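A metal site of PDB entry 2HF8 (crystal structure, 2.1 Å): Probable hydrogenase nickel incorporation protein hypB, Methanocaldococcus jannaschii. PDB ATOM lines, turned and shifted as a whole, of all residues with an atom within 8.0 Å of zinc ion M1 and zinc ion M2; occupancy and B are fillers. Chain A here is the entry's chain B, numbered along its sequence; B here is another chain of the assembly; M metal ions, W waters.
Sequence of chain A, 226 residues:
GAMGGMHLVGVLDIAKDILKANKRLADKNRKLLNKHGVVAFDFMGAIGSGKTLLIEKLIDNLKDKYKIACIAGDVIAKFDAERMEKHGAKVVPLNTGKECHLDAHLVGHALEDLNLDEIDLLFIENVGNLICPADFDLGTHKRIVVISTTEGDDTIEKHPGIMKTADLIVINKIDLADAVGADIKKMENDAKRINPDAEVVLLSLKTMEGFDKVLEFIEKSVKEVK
Along chain A the residues within 4 Å of zinc ion M1 span positions 100 to 132. The nearest printed residue that does not touch zinc ion M1 is Cys 100 of chain B (4.3 Å).
O of Cys 100 of chain A lies within hydrogen-bond range of ND2 of Asn 129 of chain A, at 3.1 Å. A ring nitrogen (NE2) of His 101 of chain A sits close to the side-chain carboxylate (OE2) of Glu 99 of chain A (3.3 Å). N of Cys 132 of chain B sits at hydrogen-bond distance from OD1 of Asn 129 of chain B (3.4 Å). The side-chain sulfur (SG) of Cys 132 of chain A sits close to the side-chain amide nitrogen (ND2) of Asn 129 of chain A, at 3.6 Å. ND2 of Asn 129 of chain B lies within hydrogen-bond range of O of Cys 100 of chain B.
Zinc ion M1 is bound by SG of Cys 100 of chain A, ND1 of His 101 of chain A, water W1 and SG of Cys 132 of chain A.
Three residues have an atom within 4 Å of zinc ion M2: Cys 100 of chain A, Cys 100 of chain B and Cys 132 of chain B.
Zinc ion M2 is bound by SG of Cys 132 of chain B (2.2 Å), SG of Cys 100 of chain A (2.2 Å) and SG of Cys 100 of chain B (2.4 Å).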
ATOM      1  N   LYS A  98      16.648  22.780 -21.735  1.00  0.00           N
ATOM      2  CA  LYS A  98      15.535  22.902 -22.668  1.00  0.00           C
ATOM      3  C   LYS A  98      15.042  21.523 -23.102  1.00  0.00           C
ATOM      4  O   LYS A  98      14.088  21.408 -23.874  1.00  0.00           O
ATOM      5  CB  LYS A  98      15.910  23.771 -23.871  1.00  0.00           C
ATOM      6  CG  LYS A  98      15.758  25.259 -23.615  1.00  0.00           C
ATOM      7  CD  LYS A  98      15.968  26.068 -24.877  1.00  0.00           C
ATOM      8  CE  LYS A  98      15.603  27.538 -24.679  1.00  0.00           C
ATOM      9  NZ  LYS A  98      16.455  28.234 -23.674  1.00  0.00           N
ATOM     10  N   GLU A  99      15.712  20.485 -22.594  1.00  0.00           N
ATOM     11  CA  GLU A  99      15.298  19.105 -22.810  1.00  0.00           C
ATOM     12  C   GLU A  99      14.053  18.824 -21.983  1.00  0.00           C
ATOM     13  O   GLU A  99      13.905  19.319 -20.869  1.00  0.00           O
ATOM     14  CB  GLU A  99      16.433  18.138 -22.464  1.00  0.00           C
ATOM     15  CG  GLU A  99      16.310  16.751 -23.097  1.00  0.00           C
ATOM     16  CD  GLU A  99      16.543  16.737 -24.594  1.00  0.00           C
ATOM     17  OE1 GLU A  99      17.282  17.613 -25.117  1.00  0.00           O
ATOM     18  OE2 GLU A  99      15.989  15.838 -25.274  1.00  0.00           O
ATOM     19  N   CYS A 100      13.163  18.009 -22.540  1.00  0.00           N
ATOM     20  CA  CYS A 100      11.805  17.847 -22.018  1.00  0.00           C
ATOM     21  C   CYS A 100      11.586  16.492 -21.368  1.00  0.00           C
ATOM     22  O   CYS A 100      10.451  16.135 -21.041  1.00  0.00           O
ATOM     23  CB  CYS A 100      10.808  18.058 -23.151  1.00  0.00           C
ATOM     24  SG  CYS A 100      11.455  17.537 -24.769  1.00  0.00           S
ATOM     25  N   HIS A 101      12.675  15.746 -21.171  1.00  0.00           N
ATOM     26  CA  HIS A 101      12.624  14.411 -20.593  1.00  0.00           C
ATOM     27  C   HIS A 101      13.986  14.003 -20.041  1.00  0.00           C
ATOM     28  O   HIS A 101      15.030  14.454 -20.532  1.00  0.00           O
ATOM     29  CB  HIS A 101      12.172  13.389 -21.651  1.00  0.00           C
ATOM     30  CG  HIS A 101      13.056  13.333 -22.856  1.00  0.00           C
ATOM     31  ND1 HIS A 101      12.745  13.968 -24.036  1.00  0.00           N
ATOM     32  CD2 HIS A 101      14.252  12.718 -23.064  1.00  0.00           C
ATOM     33  CE1 HIS A 101      13.707  13.759 -24.919  1.00  0.00           C
ATOM     34  NE2 HIS A 101      14.635  13.005 -24.343  1.00  0.00           N
ATOM     35  N   LEU A 102      13.980  13.156 -19.015  1.00  0.00           N
ATOM     36  CA  LEU A 102      15.198  12.468 -18.605  1.00  0.00           C
ATOM     37  C   LEU A 102      15.487  11.324 -19.578  1.00  0.00           C
ATOM     38  O   LEU A 102      14.572  10.835 -20.258  1.00  0.00           O
ATOM     39  CB  LEU A 102      15.079  11.938 -17.169  1.00  0.00           C
ATOM     40  CG  LEU A 102      15.076  12.945 -16.014  1.00  0.00           C
ATOM     41  CD1 LEU A 102      14.914  12.219 -14.695  1.00  0.00           C
ATOM     42  CD2 LEU A 102      16.350  13.785 -15.992  1.00  0.00           C
ATOM     43  N   VAL A 127      10.882  14.765 -15.488  1.00  0.00           N
ATOM     44  CA  VAL A 127      10.367  16.095 -15.825  1.00  0.00           C
ATOM     45  C   VAL A 127       8.847  16.042 -15.965  1.00  0.00           C
ATOM     46  O   VAL A 127       8.305  15.042 -16.450  1.00  0.00           O
ATOM     47  CB  VAL A 127      10.998  16.638 -17.153  1.00  0.00           C
ATOM     48  CG1 VAL A 127      10.693  18.113 -17.339  1.00  0.00           C
ATOM     49  CG2 VAL A 127      12.497  16.415 -17.172  1.00  0.00           C
ATOM     50  N   ASN A 129       5.745  16.209 -17.622  1.00  0.00           N
ATOM     51  CA  ASN A 129       5.528  16.001 -19.050  1.00  0.00           C
ATOM     52  C   ASN A 129       4.845  14.663 -19.264  1.00  0.00           C
ATOM     53  O   ASN A 129       5.326  13.631 -18.807  1.00  0.00           O
ATOM     54  CB  ASN A 129       6.874  16.030 -19.798  1.00  0.00           C
ATOM     55  CG  ASN A 129       6.728  16.300 -21.286  1.00  0.00           C
ATOM     56  OD1 ASN A 129       5.796  15.816 -21.939  1.00  0.00           O
ATOM     57  ND2 ASN A 129       7.658  17.072 -21.847  1.00  0.00           N
ATOM     58  N   ILE A 131       4.114  13.444 -22.367  1.00  0.00           N
ATOM     59  CA  ILE A 131       4.355  12.998 -23.738  1.00  0.00           C
ATOM     60  C   ILE A 131       5.620  12.140 -23.846  1.00  0.00           C
ATOM     61  O   ILE A 131       5.548  10.916 -23.805  1.00  0.00           O
ATOM     62  CB  ILE A 131       4.443  14.190 -24.748  1.00  0.00           C
ATOM     63  CG1 ILE A 131       3.309  15.198 -24.541  1.00  0.00           C
ATOM     64  CG2 ILE A 131       4.494  13.676 -26.197  1.00  0.00           C
ATOM     65  CD1 ILE A 131       1.912  14.611 -24.521  1.00  0.00           C
ATOM     66  N   CYS A 132       6.768  12.798 -23.980  1.00  0.00           N
ATOM     67  CA  CYS A 132       8.002  12.125 -24.368  1.00  0.00           C
ATOM     68  C   CYS A 132       8.695  11.240 -23.320  1.00  0.00           C
ATOM     69  O   CYS A 132       9.419  10.314 -23.710  1.00  0.00           O
ATOM     70  CB  CYS A 132       9.001  13.112 -24.992  1.00  0.00           C
ATOM     71  SG  CYS A 132       9.133  14.705 -24.169  1.00  0.00           S
ATOM     72  N   PRO A 133       8.487  11.492 -22.004  1.00  0.00           N
ATOM     73  CA  PRO A 133       9.022  10.522 -21.032  1.00  0.00           C
ATOM     74  C   PRO A 133       8.576   9.070 -21.246  1.00  0.00           C
ATOM     75  O   PRO A 133       9.251   8.154 -20.765  1.00  0.00           O
ATOM     76  CB  PRO A 133       8.493  11.057 -19.691  1.00  0.00           C
ATOM     77  CG  PRO A 133       8.356  12.516 -19.914  1.00  0.00           C
ATOM     78  CD  PRO A 133       7.852  12.634 -21.323  1.00  0.00           C
ATOM     79  N   ASP A 135       8.800   7.480 -23.954  1.00  0.00           N
ATOM     80  CA  ASP A 135       9.696   6.884 -24.942  1.00  0.00           C
ATOM     81  C   ASP A 135      11.080   6.558 -24.391  1.00  0.00           C
ATOM     82  O   ASP A 135      11.863   5.867 -25.058  1.00  0.00           O
ATOM     83  CB  ASP A 135       9.826   7.818 -26.155  1.00  0.00           C
ATOM     84  CG  ASP A 135       8.582   7.845 -27.022  1.00  0.00           C
ATOM     85  OD1 ASP A 135       8.260   8.929 -27.559  1.00  0.00           O
ATOM     86  OD2 ASP A 135       7.916   6.782 -27.159  1.00  0.00           O
ATOM     87  N   PHE A 136      11.388   7.065 -23.201  1.00  0.00           N
ATOM     88  CA  PHE A 136      12.753   7.000 -22.661  1.00  0.00           C
ATOM     89  C   PHE A 136      12.877   6.242 -21.336  1.00  0.00           C
ATOM     90  O   PHE A 136      12.807   6.832 -20.256  1.00  0.00           O
ATOM     91  CB  PHE A 136      13.347   8.410 -22.558  1.00  0.00           C
ATOM     92  CG  PHE A 136      13.514   9.098 -23.893  1.00  0.00           C
ATOM     93  CD1 PHE A 136      12.468   9.825 -24.451  1.00  0.00           C
ATOM     94  CD2 PHE A 136      14.714   9.005 -24.587  1.00  0.00           C
ATOM     95  CE1 PHE A 136      12.611  10.448 -25.681  1.00  0.00           C
ATOM     96  CE2 PHE A 136      14.870   9.632 -25.816  1.00  0.00           C
ATOM     97  CZ  PHE A 136      13.821  10.345 -26.374  1.00  0.00           C
ATOM     98  N   LYS B  98       3.323  11.690 -30.887  1.00  0.00           N
ATOM     99  CA  LYS B  98       4.471  11.610 -29.994  1.00  0.00           C
ATOM    100  C   LYS B  98       5.255  12.918 -29.894  1.00  0.00           C
ATOM    101  O   LYS B  98       6.175  13.043 -29.084  1.00  0.00           O
ATOM    102  CB  LYS B  98       5.394  10.441 -30.387  1.00  0.00           C
ATOM    103  CG  LYS B  98       4.854   9.071 -30.002  1.00  0.00           C
ATOM    104  CD  LYS B  98       5.924   7.993 -30.147  1.00  0.00           C
ATOM    105  CE  LYS B  98       5.467   6.686 -29.529  1.00  0.00           C
ATOM    106  NZ  LYS B  98       6.504   5.618 -29.653  1.00  0.00           N
ATOM    107  N   GLU B  99       4.878  13.901 -30.720  1.00  0.00           N
ATOM    108  CA  GLU B  99       5.527  15.213 -30.738  1.00  0.00           C
ATOM    109  C   GLU B  99       5.147  16.029 -29.498  1.00  0.00           C
ATOM    110  O   GLU B  99       4.001  16.014 -29.051  1.00  0.00           O
ATOM    111  CB  GLU B  99       5.149  15.974 -32.001  1.00  0.00           C
ATOM    112  CG  GLU B  99       6.102  17.118 -32.366  1.00  0.00           C
ATOM    113  CD  GLU B  99       7.136  16.726 -33.418  1.00  0.00           C
ATOM    114  OE1 GLU B  99       7.576  15.547 -33.455  1.00  0.00           O
ATOM    115  OE2 GLU B  99       7.508  17.619 -34.217  1.00  0.00           O
ATOM    116  N   CYS B 100       6.121  16.748 -28.938  1.00  0.00           N
ATOM    117  CA  CYS B 100       5.931  17.485 -27.691  1.00  0.00           C
ATOM    118  C   CYS B 100       5.618  18.968 -27.912  1.00  0.00           C
ATOM    119  O   CYS B 100       5.582  19.752 -26.959  1.00  0.00           O
ATOM    120  CB  CYS B 100       7.149  17.305 -26.779  1.00  0.00           C
ATOM    121  SG  CYS B 100       8.753  17.454 -27.616  1.00  0.00           S
ATOM    122  N   HIS B 101       5.374  19.342 -29.160  1.00  0.00           N
ATOM    123  CA  HIS B 101       5.102  20.731 -29.544  1.00  0.00           C
ATOM    124  C   HIS B 101       4.429  20.814 -30.914  1.00  0.00           C
ATOM    125  O   HIS B 101       4.513  19.882 -31.709  1.00  0.00           O
ATOM    126  CB  HIS B 101       6.417  21.537 -29.576  1.00  0.00           C
ATOM    127  CG  HIS B 101       7.369  21.071 -30.629  1.00  0.00           C
ATOM    128  ND1 HIS B 101       8.288  20.056 -30.409  1.00  0.00           N
ATOM    129  CD2 HIS B 101       7.528  21.455 -31.919  1.00  0.00           C
ATOM    130  CE1 HIS B 101       8.973  19.850 -31.515  1.00  0.00           C
ATOM    131  NE2 HIS B 101       8.533  20.678 -32.449  1.00  0.00           N
ATOM    132  N   ASN B 129       2.272  21.736 -22.271  1.00  0.00           N
ATOM    133  CA  ASN B 129       3.732  21.606 -22.163  1.00  0.00           C
ATOM    134  C   ASN B 129       4.311  22.989 -21.864  1.00  0.00           C
ATOM    135  O   ASN B 129       4.089  23.931 -22.622  1.00  0.00           O
ATOM    136  CB  ASN B 129       4.309  21.051 -23.477  1.00  0.00           C
ATOM    137  CG  ASN B 129       5.776  20.627 -23.364  1.00  0.00           C
ATOM    138  OD1 ASN B 129       6.525  21.134 -22.531  1.00  0.00           O
ATOM    139  ND2 ASN B 129       6.176  19.705 -24.223  1.00  0.00           N
ATOM    140  N   ILE B 131       7.553  23.654 -21.646  1.00  0.00           N
ATOM    141  CA  ILE B 131       8.950  23.654 -22.056  1.00  0.00           C
ATOM    142  C   ILE B 131       9.100  23.919 -23.556  1.00  0.00           C
ATOM    143  O   ILE B 131       9.461  25.029 -23.952  1.00  0.00           O
ATOM    144  CB  ILE B 131       9.671  22.338 -21.633  1.00  0.00           C
ATOM    145  CG1 ILE B 131       9.607  22.183 -20.103  1.00  0.00           C
ATOM    146  CG2 ILE B 131      11.124  22.336 -22.126  1.00  0.00           C
ATOM    147  CD1 ILE B 131      10.043  20.842 -19.562  1.00  0.00           C
ATOM    148  N   CYS B 132       8.808  22.918 -24.374  1.00  0.00           N
ATOM    149  CA  CYS B 132       9.121  22.920 -25.810  1.00  0.00           C
ATOM    150  C   CYS B 132       8.469  24.049 -26.633  1.00  0.00           C
ATOM    151  O   CYS B 132       9.127  24.631 -27.497  1.00  0.00           O
ATOM    152  CB  CYS B 132       8.825  21.551 -26.436  1.00  0.00           C
ATOM    153  SG  CYS B 132       9.122  20.165 -25.310  1.00  0.00           S
ATOM    154  N   PRO B 133       7.167  24.349 -26.397  1.00  0.00           N
ATOM    155  CA  PRO B 133       6.534  25.430 -27.171  1.00  0.00           C
ATOM    156  C   PRO B 133       7.202  26.819 -27.115  1.00  0.00           C
ATOM    157  O   PRO B 133       6.905  27.670 -27.949  1.00  0.00           O
ATOM    158  CB  PRO B 133       5.111  25.491 -26.580  1.00  0.00           C
ATOM    159  CG  PRO B 133       4.883  24.114 -26.051  1.00  0.00           C
ATOM    160  CD  PRO B 133       6.207  23.709 -25.483  1.00  0.00           C
ATOM    161  N   ASP B 135      10.204  27.592 -27.927  1.00  0.00           N
ATOM    162  CA  ASP B 135      11.111  27.765 -29.082  1.00  0.00           C
ATOM    163  C   ASP B 135      10.399  27.778 -30.446  1.00  0.00           C
ATOM    164  O   ASP B 135      11.024  28.103 -31.459  1.00  0.00           O
ATOM    165  CB  ASP B 135      12.173  26.670 -29.099  1.00  0.00           C
ATOM    166  CG  ASP B 135      12.964  26.591 -27.792  1.00  0.00           C
ATOM    167  OD1 ASP B 135      13.387  27.646 -27.269  1.00  0.00           O
ATOM    168  OD2 ASP B 135      13.173  25.448 -27.311  1.00  0.00           O
ATOM    169  N   PHE B 136       9.114  27.439 -30.475  1.00  0.00           N
ATOM    170  CA  PHE B 136       8.405  27.234 -31.739  1.00  0.00           C
ATOM    171  C   PHE B 136       7.274  28.230 -32.034  1.00  0.00           C
ATOM    172  O   PHE B 136       6.102  27.946 -31.816  1.00  0.00           O
ATOM    173  CB  PHE B 136       7.909  25.782 -31.841  1.00  0.00           C
ATOM    174  CG  PHE B 136       9.009  24.784 -31.993  1.00  0.00           C
ATOM    175  CD1 PHE B 136       9.562  24.157 -30.876  1.00  0.00           C
ATOM    176  CD2 PHE B 136       9.507  24.456 -33.262  1.00  0.00           C
ATOM    177  CE1 PHE B 136      10.599  23.227 -31.022  1.00  0.00           C
ATOM    178  CE2 PHE B 136      10.545  23.526 -33.408  1.00  0.00           C
ATOM    179  CZ  PHE B 136      11.088  22.908 -32.292  1.00  0.00           C
HETATM  180 ZN    ZN M   1      11.273  15.449 -24.715  1.00  0.00          ZN
HETATM  181 ZN    ZN M   2      10.357  18.651 -26.322  1.00  0.00          ZN
HETATM  182  O   HOH W   1      11.308  15.333 -26.930  1.00  0.00           O
